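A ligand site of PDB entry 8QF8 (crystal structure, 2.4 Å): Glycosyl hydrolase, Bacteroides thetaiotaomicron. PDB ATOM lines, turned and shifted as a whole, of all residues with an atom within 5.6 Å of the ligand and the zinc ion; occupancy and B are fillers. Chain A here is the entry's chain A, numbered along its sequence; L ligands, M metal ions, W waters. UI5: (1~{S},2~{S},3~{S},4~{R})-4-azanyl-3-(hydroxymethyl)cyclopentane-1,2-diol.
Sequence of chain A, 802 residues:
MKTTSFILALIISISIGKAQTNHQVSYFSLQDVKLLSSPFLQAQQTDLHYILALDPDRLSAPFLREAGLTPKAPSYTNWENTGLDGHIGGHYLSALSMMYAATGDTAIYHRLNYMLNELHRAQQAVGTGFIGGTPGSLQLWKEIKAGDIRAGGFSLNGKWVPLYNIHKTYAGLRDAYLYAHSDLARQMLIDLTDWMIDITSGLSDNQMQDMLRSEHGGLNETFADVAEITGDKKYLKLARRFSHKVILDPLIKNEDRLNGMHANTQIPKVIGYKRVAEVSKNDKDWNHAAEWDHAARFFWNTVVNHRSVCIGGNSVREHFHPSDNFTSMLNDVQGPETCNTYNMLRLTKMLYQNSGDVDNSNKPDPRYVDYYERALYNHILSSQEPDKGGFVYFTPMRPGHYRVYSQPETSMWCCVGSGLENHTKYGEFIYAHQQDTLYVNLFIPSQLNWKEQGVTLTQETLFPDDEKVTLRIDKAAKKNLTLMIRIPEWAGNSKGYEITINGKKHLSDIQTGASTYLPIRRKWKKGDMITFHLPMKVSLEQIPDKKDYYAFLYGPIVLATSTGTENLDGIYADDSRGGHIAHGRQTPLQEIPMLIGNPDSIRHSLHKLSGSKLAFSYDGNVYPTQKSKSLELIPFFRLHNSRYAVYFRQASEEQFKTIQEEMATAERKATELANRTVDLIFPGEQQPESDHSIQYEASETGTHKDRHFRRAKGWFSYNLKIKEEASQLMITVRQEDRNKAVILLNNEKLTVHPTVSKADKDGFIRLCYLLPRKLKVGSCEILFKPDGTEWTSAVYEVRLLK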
ATOM      1  N   TRP A  79      21.803  16.877  -7.022  1.00  0.00           N
ATOM      2  CA  TRP A  79      23.143  17.258  -6.591  1.00  0.00           C
ATOM      3  C   TRP A  79      23.984  17.784  -7.758  1.00  0.00           C
ATOM      4  O   TRP A  79      25.030  18.385  -7.524  1.00  0.00           O
ATOM      5  CB  TRP A  79      23.866  16.075  -5.935  1.00  0.00           C
ATOM      6  CG  TRP A  79      23.222  15.531  -4.693  1.00  0.00           C
ATOM      7  CD1 TRP A  79      21.998  15.811  -4.145  1.00  0.00           C
ATOM      8  CD2 TRP A  79      23.835  14.560  -3.812  1.00  0.00           C
ATOM      9  NE1 TRP A  79      21.811  15.076  -3.003  1.00  0.00           N
ATOM     10  CE2 TRP A  79      22.917  14.294  -2.776  1.00  0.00           C
ATOM     11  CE3 TRP A  79      25.070  13.899  -3.804  1.00  0.00           C
ATOM     12  CZ2 TRP A  79      23.191  13.392  -1.753  1.00  0.00           C
ATOM     13  CZ3 TRP A  79      25.357  13.023  -2.779  1.00  0.00           C
ATOM     14  CH2 TRP A  79      24.409  12.754  -1.779  1.00  0.00           C
ATOM     15  N   LEU A  84      27.650  19.551  -6.343  1.00  0.00           N
ATOM     16  CA  LEU A  84      28.447  18.386  -6.735  1.00  0.00           C
ATOM     17  C   LEU A  84      28.388  18.165  -8.252  1.00  0.00           C
ATOM     18  O   LEU A  84      28.656  17.061  -8.710  1.00  0.00           O
ATOM     19  CB  LEU A  84      28.017  17.159  -5.924  1.00  0.00           C
ATOM     20  CG  LEU A  84      28.908  16.830  -4.726  1.00  0.00           C
ATOM     21  CD1 LEU A  84      28.301  15.701  -3.895  1.00  0.00           C
ATOM     22  CD2 LEU A  84      30.312  16.435  -5.178  1.00  0.00           C
ATOM     23  N   TRP A 160      31.295  22.340  -2.457  1.00  0.00           N
ATOM     24  CA  TRP A 160      30.896  21.084  -1.842  1.00  0.00           C
ATOM     25  C   TRP A 160      31.839  19.961  -2.304  1.00  0.00           C
ATOM     26  O   TRP A 160      31.821  19.570  -3.465  1.00  0.00           O
ATOM     27  CB  TRP A 160      29.426  20.812  -2.207  1.00  0.00           C
ATOM     28  CG  TRP A 160      28.790  19.636  -1.514  1.00  0.00           C
ATOM     29  CD1 TRP A 160      29.226  18.973  -0.397  1.00  0.00           C
ATOM     30  CD2 TRP A 160      27.575  18.964  -1.912  1.00  0.00           C
ATOM     31  NE1 TRP A 160      28.381  17.952  -0.076  1.00  0.00           N
ATOM     32  CE2 TRP A 160      27.357  17.915  -0.993  1.00  0.00           C
ATOM     33  CE3 TRP A 160      26.653  19.157  -2.961  1.00  0.00           C
ATOM     34  CZ2 TRP A 160      26.260  17.054  -1.105  1.00  0.00           C
ATOM     35  CZ3 TRP A 160      25.564  18.307  -3.058  1.00  0.00           C
ATOM     36  CH2 TRP A 160      25.371  17.275  -2.138  1.00  0.00           C
ATOM     37  N   VAL A 161      32.701  19.508  -1.366  1.00  0.00           N
ATOM     38  CA  VAL A 161      33.653  18.408  -1.489  1.00  0.00           C
ATOM     39  C   VAL A 161      34.255  18.328  -2.900  1.00  0.00           C
ATOM     40  O   VAL A 161      34.189  17.298  -3.551  1.00  0.00           O
ATOM     41  CB  VAL A 161      33.045  17.056  -1.026  1.00  0.00           C
ATOM     42  CG1 VAL A 161      32.750  17.084   0.460  1.00  0.00           C
ATOM     43  CG2 VAL A 161      31.794  16.625  -1.778  1.00  0.00           C
ATOM     44  N   TYR A 164      36.568  15.271  -3.596  1.00  0.00           N
ATOM     45  CA  TYR A 164      35.755  14.077  -3.802  1.00  0.00           C
ATOM     46  C   TYR A 164      35.219  14.047  -5.234  1.00  0.00           C
ATOM     47  O   TYR A 164      35.191  12.996  -5.854  1.00  0.00           O
ATOM     48  CB  TYR A 164      34.626  13.988  -2.755  1.00  0.00           C
ATOM     49  CG  TYR A 164      33.538  12.939  -2.983  1.00  0.00           C
ATOM     50  CD1 TYR A 164      32.514  13.143  -3.903  1.00  0.00           C
ATOM     51  CD2 TYR A 164      33.536  11.750  -2.263  1.00  0.00           C
ATOM     52  CE1 TYR A 164      31.552  12.169  -4.133  1.00  0.00           C
ATOM     53  CE2 TYR A 164      32.558  10.779  -2.460  1.00  0.00           C
ATOM     54  CZ  TYR A 164      31.568  10.990  -3.403  1.00  0.00           C
ATOM     55  OH  TYR A 164      30.608  10.040  -3.610  1.00  0.00           O
ATOM     56  N   GLU A 215      36.541  16.237   2.566  1.00  0.00           N
ATOM     57  CA  GLU A 215      36.363  14.909   1.990  1.00  0.00           C
ATOM     58  C   GLU A 215      36.884  14.941   0.563  1.00  0.00           C
ATOM     59  O   GLU A 215      36.531  15.838  -0.201  1.00  0.00           O
ATOM     60  CB  GLU A 215      34.891  14.493   2.002  1.00  0.00           C
ATOM     61  CG  GLU A 215      34.645  13.116   1.431  1.00  0.00           C
ATOM     62  CD  GLU A 215      33.202  12.636   1.376  1.00  0.00           C
ATOM     63  OE1 GLU A 215      32.293  13.425   1.698  1.00  0.00           O
ATOM     64  OE2 GLU A 215      33.004  11.471   0.982  1.00  0.00           O
ATOM     65  N   HIS A 262      32.269  10.402   9.580  1.00  0.00           N
ATOM     66  CA  HIS A 262      31.533  10.078   8.377  1.00  0.00           C
ATOM     67  C   HIS A 262      32.272   8.931   7.700  1.00  0.00           C
ATOM     68  O   HIS A 262      33.456   9.066   7.401  1.00  0.00           O
ATOM     69  CB  HIS A 262      31.386  11.343   7.517  1.00  0.00           C
ATOM     70  CG  HIS A 262      30.591  11.124   6.276  1.00  0.00           C
ATOM     71  ND1 HIS A 262      31.181  10.600   5.144  1.00  0.00           N
ATOM     72  CD2 HIS A 262      29.308  11.330   5.963  1.00  0.00           C
ATOM     73  CE1 HIS A 262      30.262  10.501   4.196  1.00  0.00           C
ATOM     74  NE2 HIS A 262      29.120  10.945   4.668  1.00  0.00           N
ATOM     75  N   ASN A 264      31.873   6.841   4.787  1.00  0.00           N
ATOM     76  CA  ASN A 264      32.254   6.751   3.387  1.00  0.00           C
ATOM     77  C   ASN A 264      33.391   7.722   3.044  1.00  0.00           C
ATOM     78  O   ASN A 264      34.060   7.526   2.032  1.00  0.00           O
ATOM     79  CB  ASN A 264      31.072   6.986   2.442  1.00  0.00           C
ATOM     80  CG  ASN A 264      31.335   6.422   1.055  1.00  0.00           C
ATOM     81  OD1 ASN A 264      31.657   5.242   0.924  1.00  0.00           O
ATOM     82  ND2 ASN A 264      31.283   7.259   0.030  1.00  0.00           N
ATOM     83  N   THR A 265      33.591   8.781   3.841  1.00  0.00           N
ATOM     84  CA  THR A 265      34.773   9.620   3.707  1.00  0.00           C
ATOM     85  C   THR A 265      36.038   8.786   3.919  1.00  0.00           C
ATOM     86  O   THR A 265      36.998   8.950   3.168  1.00  0.00           O
ATOM     87  CB  THR A 265      34.718  10.816   4.673  1.00  0.00           C
ATOM     88  OG1 THR A 265      33.614  11.654   4.314  1.00  0.00           O
ATOM     89  CG2 THR A 265      35.990  11.643   4.669  1.00  0.00           C
ATOM     90  N   GLU A 318      25.008   7.861   7.782  1.00  0.00           N
ATOM     91  CA  GLU A 318      26.298   7.978   7.104  1.00  0.00           C
ATOM     92  C   GLU A 318      27.495   7.981   8.054  1.00  0.00           C
ATOM     93  O   GLU A 318      28.618   8.175   7.590  1.00  0.00           O
ATOM     94  CB  GLU A 318      26.354   9.243   6.223  1.00  0.00           C
ATOM     95  CG  GLU A 318      25.140   9.474   5.325  1.00  0.00           C
ATOM     96  CD  GLU A 318      25.312  10.633   4.372  1.00  0.00           C
ATOM     97  OE1 GLU A 318      26.352  11.305   4.416  1.00  0.00           O
ATOM     98  OE2 GLU A 318      24.405  10.856   3.586  1.00  0.00           O
ATOM     99  N   GLU A 337      24.653   2.835   4.467  1.00  0.00           N
ATOM    100  CA  GLU A 337      24.725   3.456   3.160  1.00  0.00           C
ATOM    101  C   GLU A 337      25.391   2.494   2.174  1.00  0.00           C
ATOM    102  O   GLU A 337      26.330   1.789   2.549  1.00  0.00           O
ATOM    103  CB  GLU A 337      25.528   4.758   3.271  1.00  0.00           C
ATOM    104  CG  GLU A 337      25.707   5.461   1.944  1.00  0.00           C
ATOM    105  CD  GLU A 337      26.601   6.674   1.958  1.00  0.00           C
ATOM    106  OE1 GLU A 337      27.038   7.092   0.850  1.00  0.00           O
ATOM    107  OE2 GLU A 337      26.887   7.187   3.060  1.00  0.00           O
ATOM    108  N   THR A 338      24.936   2.495   0.914  1.00  0.00           N
ATOM    109  CA  THR A 338      25.405   1.553  -0.082  1.00  0.00           C
ATOM    110  C   THR A 338      26.857   1.832  -0.509  1.00  0.00           C
ATOM    111  O   THR A 338      27.617   0.877  -0.689  1.00  0.00           O
ATOM    112  CB  THR A 338      24.473   1.490  -1.299  1.00  0.00           C
ATOM    113  OG1 THR A 338      23.119   1.570  -0.850  1.00  0.00           O
ATOM    114  CG2 THR A 338      24.638   0.217  -2.089  1.00  0.00           C
ATOM    115  N   CYS A 339      27.248   3.114  -0.645  1.00  0.00           N
ATOM    116  CA  CYS A 339      28.612   3.443  -1.028  1.00  0.00           C
ATOM    117  C   CYS A 339      29.644   2.752  -0.131  1.00  0.00           C
ATOM    118  O   CYS A 339      30.692   2.295  -0.608  1.00  0.00           O
ATOM    119  CB  CYS A 339      28.896   4.952  -0.979  1.00  0.00           C
ATOM    120  SG  CYS A 339      28.199   5.919  -2.301  1.00  0.00           S
ATOM    121  N   ASN A 340      29.340   2.681   1.174  1.00  0.00           N
ATOM    122  CA  ASN A 340      30.266   2.151   2.155  1.00  0.00           C
ATOM    123  C   ASN A 340      30.589   0.695   1.838  1.00  0.00           C
ATOM    124  O   ASN A 340      31.743   0.301   1.923  1.00  0.00           O
ATOM    125  CB  ASN A 340      29.746   2.308   3.587  1.00  0.00           C
ATOM    126  CG  ASN A 340      29.232   3.690   3.915  1.00  0.00           C
ATOM    127  OD1 ASN A 340      28.925   4.487   3.033  1.00  0.00           O
ATOM    128  ND2 ASN A 340      29.084   3.971   5.203  1.00  0.00           N
ATOM    129  N   TYR A 393      20.035   4.174  -1.410  1.00  0.00           N
ATOM    130  CA  TYR A 393      21.026   4.922  -0.647  1.00  0.00           C
ATOM    131  C   TYR A 393      21.116   4.330   0.750  1.00  0.00           C
ATOM    132  O   TYR A 393      22.182   3.888   1.169  1.00  0.00           O
ATOM    133  CB  TYR A 393      20.632   6.402  -0.704  1.00  0.00           C
ATOM    134  CG  TYR A 393      21.632   7.445  -0.236  1.00  0.00           C
ATOM    135  CD1 TYR A 393      22.193   7.417   1.036  1.00  0.00           C
ATOM    136  CD2 TYR A 393      21.980   8.519  -1.058  1.00  0.00           C
ATOM    137  CE1 TYR A 393      23.088   8.390   1.463  1.00  0.00           C
ATOM    138  CE2 TYR A 393      22.873   9.501  -0.636  1.00  0.00           C
ATOM    139  CZ  TYR A 393      23.426   9.441   0.623  1.00  0.00           C
ATOM    140  OH  TYR A 393      24.285  10.437   1.001  1.00  0.00           O
ATOM    141  N   CYS A 414      25.446  10.091  -4.351  1.00  0.00           N
ATOM    142  CA  CYS A 414      26.663   9.309  -4.279  1.00  0.00           C
ATOM    143  C   CYS A 414      26.355   7.826  -4.505  1.00  0.00           C
ATOM    144  O   CYS A 414      27.098   7.135  -5.198  1.00  0.00           O
ATOM    145  CB  CYS A 414      27.402   9.504  -2.950  1.00  0.00           C
ATOM    146  SG  CYS A 414      26.495   9.431  -1.413  1.00  0.00           S
ATOM    147  N   CYS A 415      25.246   7.352  -3.900  1.00  0.00           N
ATOM    148  CA  CYS A 415      24.859   5.951  -4.005  1.00  0.00           C
ATOM    149  C   CYS A 415      24.307   5.593  -5.394  1.00  0.00           C
ATOM    150  O   CYS A 415      24.232   4.400  -5.720  1.00  0.00           O
ATOM    151  CB  CYS A 415      23.877   5.598  -2.888  1.00  0.00           C
ATOM    152  SG  CYS A 415      24.628   5.578  -1.276  1.00  0.00           S
ATOM    153  N   SER A 418      28.037   5.040  -7.235  1.00  0.00           N
ATOM    154  CA  SER A 418      28.529   3.713  -6.897  1.00  0.00           C
ATOM    155  C   SER A 418      27.571   2.620  -7.368  1.00  0.00           C
ATOM    156  O   SER A 418      28.011   1.524  -7.714  1.00  0.00           O
ATOM    157  CB  SER A 418      28.799   3.601  -5.419  1.00  0.00           C
ATOM    158  OG  SER A 418      27.638   3.936  -4.692  1.00  0.00           O
ATOM    159  N   GLN A 686      27.099  16.159   7.589  1.00  0.00           N
ATOM    160  CA  GLN A 686      27.362  16.886   6.357  1.00  0.00           C
ATOM    161  C   GLN A 686      26.161  16.856   5.401  1.00  0.00           C
ATOM    162  O   GLN A 686      25.772  17.899   4.878  1.00  0.00           O
ATOM    163  CB  GLN A 686      28.669  16.451   5.681  1.00  0.00           C
ATOM    164  CG  GLN A 686      28.785  14.979   5.357  1.00  0.00           C
ATOM    165  CD  GLN A 686      30.132  14.668   4.723  1.00  0.00           C
ATOM    166  OE1 GLN A 686      31.179  14.909   5.318  1.00  0.00           O
ATOM    167  NE2 GLN A 686      30.104  14.144   3.511  1.00  0.00           N
ATOM    168  N   GLN A 687      25.518  15.689   5.216  1.00  0.00           N
ATOM    169  CA  GLN A 687      24.440  15.576   4.247  1.00  0.00           C
ATOM    170  C   GLN A 687      23.160  16.285   4.710  1.00  0.00           C
ATOM    171  O   GLN A 687      22.571  17.021   3.920  1.00  0.00           O
ATOM    172  CB  GLN A 687      24.196  14.114   3.838  1.00  0.00           C
ATOM    173  CG  GLN A 687      23.554  13.967   2.450  1.00  0.00           C
ATOM    174  CD  GLN A 687      24.280  14.753   1.385  1.00  0.00           C
ATOM    175  OE1 GLN A 687      25.517  14.755   1.331  1.00  0.00           O
ATOM    176  NE2 GLN A 687      23.552  15.488   0.567  1.00  0.00           N
HETATM  177  C6  UI5 L   1      30.306  13.032  -0.660  1.00  0.00           C
HETATM  178  C5  UI5 L   1      29.513  11.731  -0.644  1.00  0.00           C
HETATM  179  C1  UI5 L   1      27.982  11.862  -0.755  1.00  0.00           C
HETATM  180  C2  UI5 L   1      27.363  10.541  -0.187  1.00  0.00           C
HETATM  181  C3  UI5 L   1      28.536   9.907   0.606  1.00  0.00           C
HETATM  182  O3  UI5 L   1      30.017  13.827   0.480  1.00  0.00           O
HETATM  183  C4  UI5 L   1      29.722  10.884   0.617  1.00  0.00           C
HETATM  184  O2  UI5 L   1      30.920  10.112   0.587  1.00  0.00           O
HETATM  185  N1  UI5 L   1      27.440  13.079  -0.076  1.00  0.00           N
HETATM  186  O1  UI5 L   1      28.252   9.586   1.976  1.00  0.00           O
HETATM  187 ZN    ZN M   1      26.444   6.924  -1.069  1.00  0.00          ZN
HETATM  188  O   HOH W   1      27.550  13.060   2.795  1.00  0.00           O
HETATM  189  O   HOH W   2      28.215  15.888   1.561  1.00  0.00           O
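A nitrogen (N1) of the ligand sits at hydrogen-bond distance from the side-chain amide oxygen (OE1) of Gln 687, at 2.9 Å. A carbon (C2) of the ligand is covalently linked to the side-chain sulfur of Cys 414 (1.9 Å). An oxygen (O2) of the ligand lies within hydrogen-bond range of the side-chain amide nitrogen of Asn 264 (2.9 Å). The side-chain amide nitrogen (NE2) of Gln 686 is in hydrogen-bond range of an oxygen (O3) of the ligand (3.0 Å). The side-chain carboxylate of Glu 337 is in hydrogen-bond range of an oxygen (O1) of the ligand (3.0 Å). The side-chain carboxylate of Glu 215 is in hydrogen-bond range of an oxygen (O2) of the ligand (2.5 Å). A ring nitrogen (NE2) of His 262 lies close to an oxygen (O1) of the ligand, 3.1 Å away.
The side-chain hydroxyl (OG1) of Thr 265 is in hydrogen-bond range of a ring nitrogen (ND1) of His 262. O of Cys 414 is in hydrogen-bond range of OG of Ser 418 (3.3 Å). The side-chain carboxylate (OE2) of Glu 215 sits close to the side-chain hydroxyl (OG1) of Thr 265 (3.4 Å). A ring nitrogen (NE2) of His 262 sits at hydrogen-bond distance from the side-chain carboxylate (OE1) of Glu 318 (2.8 Å). The side-chain sulfur of Cys 414 lies close to the side-chain hydroxyl of Tyr 393 (3.4 Å). O of Tyr 393 is in hydrogen-bond range of N of Thr 338 (3.1 Å). The backbone NH (N) of Thr 338 sits close to the side-chain sulfur (SG) of Cys 415 (3.8 Å). O of Glu 215 is in hydrogen-bond range of N of Tyr 164, 3.4 Å away.
Trp 79 touches the ligand (CZ3 to N1, 3.4 Å). Tyr 164 touches the ligand (CZ to C5, 3.5 Å). Glu 318 touches the ligand (OE1 to O1, 3.5 Å). Tyr 393 touches the ligand (OH to C2, 3.3 Å). Hydrophobic or aromatic side chains that line the ligand: Trp 79, Tyr 164 and His 262. The nearest printed residue that does not touch the ligand is Val 161 (4.01 Å).
The zinc ion is bound by OE1 of Glu 337 (2.0 Å), SG of Cys 415 (2.3 Å), SG of Cys 339 (2.4 Å) and SG of Cys 414 (2.5 Å). The zinc ion has four donor atoms within binding distance.
Water W1 lies within hydrogen-bond range of the side-chain carboxylate (OE1) of Glu 318 (2.7 Å), the side-chain amide nitrogen (NE2) of Gln 686 (2.9 Å), a nitrogen (N1) of the ligand (2.9 Å), the side-chain amide oxygen (OE1) of Gln 687 (3.0 Å) and a ring nitrogen (NE2) of His 262 (3.2 Å). Water W2 lies within hydrogen-bond range of the indole nitrogen (NE1) of Trp 160 (2.6 Å), the side-chain amide oxygen (OE1) of Gln 687 (2.9 Å), an oxygen (O3) of the ligand (2.9 Å) and the side-chain amide nitrogen (NE2) of Gln 686 (3.2 Å).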
